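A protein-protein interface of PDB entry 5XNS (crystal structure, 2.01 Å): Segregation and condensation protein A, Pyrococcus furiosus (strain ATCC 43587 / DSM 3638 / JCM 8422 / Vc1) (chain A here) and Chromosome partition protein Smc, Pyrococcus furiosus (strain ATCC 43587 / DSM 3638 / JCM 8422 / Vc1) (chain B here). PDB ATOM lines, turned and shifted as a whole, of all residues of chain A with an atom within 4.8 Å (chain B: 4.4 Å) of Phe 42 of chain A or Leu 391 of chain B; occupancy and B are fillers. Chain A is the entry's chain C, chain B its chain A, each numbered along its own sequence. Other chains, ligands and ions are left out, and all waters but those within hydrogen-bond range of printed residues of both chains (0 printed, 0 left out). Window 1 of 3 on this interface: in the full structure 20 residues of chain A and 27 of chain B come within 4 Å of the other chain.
N of Leu 391 of chain B lies within hydrogen-bond range of O of Ile 376 of chain B (2.9 Å). The backbone carbonyl oxygen of Val 389 of chain B lies within hydrogen-bond range of the backbone NH of Gly 378 of chain B (2.8 Å). N of Phe 26 of chain A sits at hydrogen-bond distance from O of Ile 65 of chain A (2.8 Å).
Leu 391 of chain B touches Phe 26 of chain A (CD1 to CE2, 3.96 Å). Trp 27 of chain A touches Leu 391 of chain B (CH2 to CD1, 3.7 Å). Leu 393 of chain B touches Ile 38 of chain A. CB of Ala 39 of chain A touches CD1 of Ile 376 of chain B (3.9 Å). Phe 42 of chain A touches Ile 376 of chain B. Phe 42 of chain A touches Gly 378 of chain B (CE2 to N, 3.7 Å). Leu 46 of chain A touches Gly 378 of chain B. CD1 of Phe 62 of chain A touches C of Leu 391 of chain B, 3.6 Å away. Ile 65 of chain A touches Val 389 of chain B. CD1 of Ile 65 of chain A touches CD1 of Leu 391 of chain B, at 3.9 Å.
Hydrophobic or aromatic side chains of chain B that line the printed part of chain A: Ile 376, Val 389, Leu 391 and Leu 393. Printed residues of chain A that touch a printed residue of chain B: Phe 26, Trp 27, Ile 38, Ala 39, Phe 42, Leu 46, Phe 62 and Ile 65. Among the printed residues, no Asp or Glu carboxylate lies within 4 Å of a Lys or Arg side-chain nitrogen of the other chain.
The backbone NH (N) of Phe 62 of chain A is in hydrogen-bond range of the side-chain hydroxyl (OG) of Ser 390 of chain B (2.8 Å).
Of chain A, only Phe 26, Trp 27, Phe 42, Phe 62 and Ile 65 come within 4 Å of Leu 391 of chain B. Of the printed residues of chain B, Ala 39 of chain A touches Ile 376. Of the printed residues of chain A, Gly 378 of chain B touches Phe 42 and Leu 46. Of the printed residues of chain A, Lys 375 of chain B touches Phe 62 (3.5 Å). Printed residues of chain A within 4 Å of Leu 393 of chain B: Ile 38. Arg 40 of chain A touches none of the printed residues of chain B. Leu 45 of chain A touches none of the printed residues of chain B. The nearest residue of chain A that does not touch Leu 391 of chain B is Ile 38 of chain A (4.02 Å). The nearest printed residue of chain A that does not touch Val 389 of chain B is Leu 46 of chain A (5.1 Å).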
ATOM      1  N   PHE A  26      23.534   8.607   0.959  1.00  0.00           N
ATOM      2  CA  PHE A  26      24.449   7.567   1.427  1.00  0.00           C
ATOM      3  C   PHE A  26      24.225   6.261   0.676  1.00  0.00           C
ATOM      4  O   PHE A  26      25.186   5.632   0.219  1.00  0.00           O
ATOM      5  CB  PHE A  26      24.299   7.348   2.942  1.00  0.00           C
ATOM      6  CG  PHE A  26      25.071   6.152   3.470  1.00  0.00           C
ATOM      7  CD1 PHE A  26      26.455   6.120   3.406  1.00  0.00           C
ATOM      8  CD2 PHE A  26      24.406   5.063   4.024  1.00  0.00           C
ATOM      9  CE1 PHE A  26      27.177   5.028   3.900  1.00  0.00           C
ATOM     10  CE2 PHE A  26      25.117   3.945   4.514  1.00  0.00           C
ATOM     11  CZ  PHE A  26      26.509   3.934   4.451  1.00  0.00           C
ATOM     12  N   TRP A  27      22.959   5.837   0.530  1.00  0.00           N
ATOM     13  CA  TRP A  27      22.688   4.550  -0.108  1.00  0.00           C
ATOM     14  C   TRP A  27      23.328   4.464  -1.487  1.00  0.00           C
ATOM     15  O   TRP A  27      23.798   3.397  -1.896  1.00  0.00           O
ATOM     16  CB  TRP A  27      21.184   4.291  -0.237  1.00  0.00           C
ATOM     17  CG  TRP A  27      20.388   4.350   1.035  1.00  0.00           C
ATOM     18  CD1 TRP A  27      19.197   5.005   1.224  1.00  0.00           C
ATOM     19  CD2 TRP A  27      20.704   3.728   2.286  1.00  0.00           C
ATOM     20  NE1 TRP A  27      18.762   4.832   2.514  1.00  0.00           N
ATOM     21  CE2 TRP A  27      19.666   4.054   3.190  1.00  0.00           C
ATOM     22  CE3 TRP A  27      21.761   2.928   2.736  1.00  0.00           C
ATOM     23  CZ2 TRP A  27      19.662   3.611   4.520  1.00  0.00           C
ATOM     24  CZ3 TRP A  27      21.757   2.502   4.051  1.00  0.00           C
ATOM     25  CH2 TRP A  27      20.712   2.840   4.929  1.00  0.00           C
ATOM     26  N   ILE A  38      28.756  -1.717   3.770  1.00  0.00           N
ATOM     27  CA  ILE A  38      27.963  -0.614   4.303  1.00  0.00           C
ATOM     28  C   ILE A  38      28.724   0.064   5.428  1.00  0.00           C
ATOM     29  O   ILE A  38      28.895   1.286   5.438  1.00  0.00           O
ATOM     30  CB  ILE A  38      26.584  -1.103   4.777  1.00  0.00           C
ATOM     31  CG1 ILE A  38      25.804  -1.723   3.617  1.00  0.00           C
ATOM     32  CG2 ILE A  38      25.791   0.060   5.348  1.00  0.00           C
ATOM     33  CD1 ILE A  38      24.645  -2.568   4.065  1.00  0.00           C
ATOM     34  N   ALA A  39      29.239  -0.729   6.366  1.00  0.00           N
ATOM     35  CA  ALA A  39      29.929  -0.144   7.507  1.00  0.00           C
ATOM     36  C   ALA A  39      31.161   0.633   7.059  1.00  0.00           C
ATOM     37  O   ALA A  39      31.391   1.766   7.505  1.00  0.00           O
ATOM     38  CB  ALA A  39      30.298  -1.243   8.503  1.00  0.00           C
ATOM     39  N   ARG A  40      31.945   0.053   6.143  1.00  0.00           N
ATOM     40  CA  ARG A  40      33.174   0.702   5.688  1.00  0.00           C
ATOM     41  C   ARG A  40      32.890   2.014   4.954  1.00  0.00           C
ATOM     42  O   ARG A  40      33.607   3.007   5.137  1.00  0.00           O
ATOM     43  CB  ARG A  40      33.952  -0.269   4.801  1.00  0.00           C
ATOM     44  CG  ARG A  40      35.288   0.253   4.309  1.00  0.00           C
ATOM     45  CD  ARG A  40      35.918  -0.746   3.343  1.00  0.00           C
ATOM     46  NE  ARG A  40      36.323  -1.988   4.004  1.00  0.00           N
ATOM     47  CZ  ARG A  40      36.572  -3.122   3.354  1.00  0.00           C
ATOM     48  NH1 ARG A  40      36.428  -3.160   2.032  1.00  0.00           N
ATOM     49  NH2 ARG A  40      36.955  -4.217   4.013  1.00  0.00           N
ATOM     50  N   THR A  41      31.854   2.040   4.116  1.00  0.00           N
ATOM     51  CA  THR A  41      31.484   3.284   3.448  1.00  0.00           C
ATOM     52  C   THR A  41      31.130   4.352   4.473  1.00  0.00           C
ATOM     53  O   THR A  41      31.610   5.490   4.396  1.00  0.00           O
ATOM     54  CB  THR A  41      30.303   3.051   2.500  1.00  0.00           C
ATOM     55  OG1 THR A  41      30.573   1.919   1.659  1.00  0.00           O
ATOM     56  CG2 THR A  41      30.048   4.302   1.629  1.00  0.00           C
ATOM     57  N   PHE A  42      30.292   3.991   5.450  1.00  0.00           N
ATOM     58  CA  PHE A  42      29.916   4.919   6.510  1.00  0.00           C
ATOM     59  C   PHE A  42      31.159   5.439   7.236  1.00  0.00           C
ATOM     60  O   PHE A  42      31.330   6.656   7.418  1.00  0.00           O
ATOM     61  CB  PHE A  42      28.951   4.211   7.465  1.00  0.00           C
ATOM     62  CG  PHE A  42      28.320   5.103   8.496  1.00  0.00           C
ATOM     63  CD1 PHE A  42      27.851   6.370   8.160  1.00  0.00           C
ATOM     64  CD2 PHE A  42      28.152   4.652   9.807  1.00  0.00           C
ATOM     65  CE1 PHE A  42      27.259   7.184   9.120  1.00  0.00           C
ATOM     66  CE2 PHE A  42      27.548   5.450  10.771  1.00  0.00           C
ATOM     67  CZ  PHE A  42      27.099   6.721  10.430  1.00  0.00           C
ATOM     68  N   LEU A  43      32.074   4.527   7.588  1.00  0.00           N
ATOM     69  CA  LEU A  43      33.286   4.903   8.315  1.00  0.00           C
ATOM     70  C   LEU A  43      34.142   5.873   7.511  1.00  0.00           C
ATOM     71  O   LEU A  43      34.604   6.894   8.036  1.00  0.00           O
ATOM     72  CB  LEU A  43      34.093   3.652   8.666  1.00  0.00           C
ATOM     73  CG  LEU A  43      35.334   3.814   9.547  1.00  0.00           C
ATOM     74  CD1 LEU A  43      34.951   4.277  10.932  1.00  0.00           C
ATOM     75  CD2 LEU A  43      36.054   2.474   9.634  1.00  0.00           C
ATOM     76  N   TYR A  44      34.371   5.563   6.232  1.00  0.00           N
ATOM     77  CA  TYR A  44      35.199   6.425   5.396  1.00  0.00           C
ATOM     78  C   TYR A  44      34.598   7.825   5.291  1.00  0.00           C
ATOM     79  O   TYR A  44      35.325   8.828   5.315  1.00  0.00           O
ATOM     80  CB  TYR A  44      35.375   5.780   4.019  1.00  0.00           C
ATOM     81  CG  TYR A  44      36.270   4.543   4.050  1.00  0.00           C
ATOM     82  CD1 TYR A  44      36.875   4.132   5.231  1.00  0.00           C
ATOM     83  CD2 TYR A  44      36.522   3.811   2.905  1.00  0.00           C
ATOM     84  CE1 TYR A  44      37.693   3.023   5.273  1.00  0.00           C
ATOM     85  CE2 TYR A  44      37.340   2.696   2.933  1.00  0.00           C
ATOM     86  CZ  TYR A  44      37.925   2.306   4.120  1.00  0.00           C
ATOM     87  OH  TYR A  44      38.741   1.189   4.161  1.00  0.00           O
ATOM     88  N   LEU A  45      33.267   7.912   5.209  1.00  0.00           N
ATOM     89  CA  LEU A  45      32.621   9.216   5.236  1.00  0.00           C
ATOM     90  C   LEU A  45      32.848   9.913   6.579  1.00  0.00           C
ATOM     91  O   LEU A  45      33.142  11.114   6.619  1.00  0.00           O
ATOM     92  CB  LEU A  45      31.135   9.063   4.926  1.00  0.00           C
ATOM     93  CG  LEU A  45      30.849   8.659   3.478  1.00  0.00           C
ATOM     94  CD1 LEU A  45      29.406   8.212   3.339  1.00  0.00           C
ATOM     95  CD2 LEU A  45      31.185   9.794   2.481  1.00  0.00           C
ATOM     96  N   LEU A  46      32.779   9.170   7.686  1.00  0.00           N
ATOM     97  CA  LEU A  46      33.026   9.814   8.976  1.00  0.00           C
ATOM     98  C   LEU A  46      34.467  10.287   9.086  1.00  0.00           C
ATOM     99  O   LEU A  46      34.732  11.335   9.690  1.00  0.00           O
ATOM    100  CB  LEU A  46      32.669   8.875  10.125  1.00  0.00           C
ATOM    101  CG  LEU A  46      31.177   8.570  10.116  1.00  0.00           C
ATOM    102  CD1 LEU A  46      30.914   7.216  10.777  1.00  0.00           C
ATOM    103  CD2 LEU A  46      30.390   9.683  10.779  1.00  0.00           C
ATOM    104  N   PHE A  62      18.372   7.516  12.498  1.00  0.00           N
ATOM    105  CA  PHE A  62      18.180   6.396  11.575  1.00  0.00           C
ATOM    106  C   PHE A  62      17.401   6.796  10.329  1.00  0.00           C
ATOM    107  O   PHE A  62      16.807   5.942   9.661  1.00  0.00           O
ATOM    108  CB  PHE A  62      17.503   5.214  12.269  1.00  0.00           C
ATOM    109  CG  PHE A  62      18.217   4.767  13.501  1.00  0.00           C
ATOM    110  CD1 PHE A  62      19.431   4.099  13.408  1.00  0.00           C
ATOM    111  CD2 PHE A  62      17.687   5.013  14.759  1.00  0.00           C
ATOM    112  CE1 PHE A  62      20.097   3.677  14.554  1.00  0.00           C
ATOM    113  CE2 PHE A  62      18.352   4.599  15.908  1.00  0.00           C
ATOM    114  CZ  PHE A  62      19.557   3.934  15.804  1.00  0.00           C
ATOM    115  N   ILE A  65      20.454   9.491   5.162  1.00  0.00           N
ATOM    116  CA  ILE A  65      21.735  10.163   5.305  1.00  0.00           C
ATOM    117  C   ILE A  65      22.150  10.718   3.944  1.00  0.00           C
ATOM    118  O   ILE A  65      22.087  10.006   2.936  1.00  0.00           O
ATOM    119  CB  ILE A  65      22.790   9.186   5.847  1.00  0.00           C
ATOM    120  CG1 ILE A  65      22.320   8.599   7.183  1.00  0.00           C
ATOM    121  CG2 ILE A  65      24.141   9.873   5.965  1.00  0.00           C
ATOM    122  CD1 ILE A  65      23.160   7.412   7.675  1.00  0.00           C
ATOM    123  N   LYS B 375      23.282  -1.812  15.072  1.00  0.00           N
ATOM    124  CA  LYS B 375      23.252  -0.396  14.754  1.00  0.00           C
ATOM    125  C   LYS B 375      24.642   0.190  14.916  1.00  0.00           C
ATOM    126  O   LYS B 375      25.477  -0.327  15.667  1.00  0.00           O
ATOM    127  CB  LYS B 375      22.227   0.351  15.615  1.00  0.00           C
ATOM    128  CG  LYS B 375      20.788   0.054  15.184  1.00  0.00           C
ATOM    129  CD  LYS B 375      19.768   0.456  16.248  1.00  0.00           C
ATOM    130  CE  LYS B 375      18.354   0.513  15.660  1.00  0.00           C
ATOM    131  NZ  LYS B 375      17.338   0.873  16.687  1.00  0.00           N
ATOM    132  N   ILE B 376      24.898   1.247  14.156  1.00  0.00           N
ATOM    133  CA  ILE B 376      26.187   1.919  14.150  1.00  0.00           C
ATOM    134  C   ILE B 376      25.931   3.395  14.368  1.00  0.00           C
ATOM    135  O   ILE B 376      25.074   3.984  13.703  1.00  0.00           O
ATOM    136  CB  ILE B 376      26.956   1.680  12.837  1.00  0.00           C
ATOM    137  CG1 ILE B 376      27.214   0.175  12.652  1.00  0.00           C
ATOM    138  CG2 ILE B 376      28.251   2.459  12.840  1.00  0.00           C
ATOM    139  CD1 ILE B 376      27.800  -0.173  11.305  1.00  0.00           C
ATOM    140  N   GLY B 378      27.822   6.840  14.204  1.00  0.00           N
ATOM    141  CA  GLY B 378      29.017   7.455  13.677  1.00  0.00           C
ATOM    142  C   GLY B 378      29.220   8.792  14.357  1.00  0.00           C
ATOM    143  O   GLY B 378      28.273   9.560  14.523  1.00  0.00           O
ATOM    144  N   VAL B 389      25.663  10.563  13.844  1.00  0.00           N
ATOM    145  CA  VAL B 389      24.759  10.107  12.799  1.00  0.00           C
ATOM    146  C   VAL B 389      24.488   8.632  13.057  1.00  0.00           C
ATOM    147  O   VAL B 389      25.428   7.868  13.317  1.00  0.00           O
ATOM    148  CB  VAL B 389      25.385  10.313  11.403  1.00  0.00           C
ATOM    149  CG1 VAL B 389      24.515   9.678  10.322  1.00  0.00           C
ATOM    150  CG2 VAL B 389      25.613  11.806  11.140  1.00  0.00           C
ATOM    151  N   SER B 390      23.223   8.221  12.978  1.00  0.00           N
ATOM    152  CA  SER B 390      22.841   6.862  13.351  1.00  0.00           C
ATOM    153  C   SER B 390      22.343   6.057  12.154  1.00  0.00           C
ATOM    154  O   SER B 390      21.576   6.553  11.318  1.00  0.00           O
ATOM    155  CB  SER B 390      21.763   6.866  14.437  1.00  0.00           C
ATOM    156  OG  SER B 390      20.679   7.698  14.062  1.00  0.00           O
ATOM    157  N   LEU B 391      22.746   4.789  12.115  1.00  0.00           N
ATOM    158  CA  LEU B 391      22.517   3.901  10.986  1.00  0.00           C
ATOM    159  C   LEU B 391      22.053   2.554  11.503  1.00  0.00           C
ATOM    160  O   LEU B 391      22.635   2.022  12.455  1.00  0.00           O
ATOM    161  CB  LEU B 391      23.803   3.729  10.171  1.00  0.00           C
ATOM    162  CG  LEU B 391      23.765   2.831   8.938  1.00  0.00           C
ATOM    163  CD1 LEU B 391      22.981   3.537   7.827  1.00  0.00           C
ATOM    164  CD2 LEU B 391      25.193   2.505   8.487  1.00  0.00           C
ATOM    165  N   SER B 392      21.020   2.002  10.883  1.00  0.00           N
ATOM    166  CA  SER B 392      20.579   0.647  11.181  1.00  0.00           C
ATOM    167  C   SER B 392      21.079  -0.277  10.081  1.00  0.00           C
ATOM    168  O   SER B 392      20.851  -0.012   8.898  1.00  0.00           O
ATOM    169  CB  SER B 392      19.055   0.572  11.285  1.00  0.00           C
ATOM    170  OG  SER B 392      18.621  -0.782  11.267  1.00  0.00           O
ATOM    171  N   LEU B 393      21.770  -1.354  10.459  1.00  0.00           N
ATOM    172  CA  LEU B 393      22.318  -2.216   9.411  1.00  0.00           C
ATOM    173  C   LEU B 393      21.236  -3.090   8.789  1.00  0.00           C
ATOM    174  O   LEU B 393      21.236  -3.308   7.570  1.00  0.00           O
ATOM    175  CB  LEU B 393      23.466  -3.067   9.948  1.00  0.00           C
ATOM    176  CG  LEU B 393      24.834  -2.392   9.810  1.00  0.00           C
ATOM    177  CD1 LEU B 393      25.948  -3.288  10.328  1.00  0.00           C
ATOM    178  CD2 LEU B 393      25.123  -1.997   8.370  1.00  0.00           C
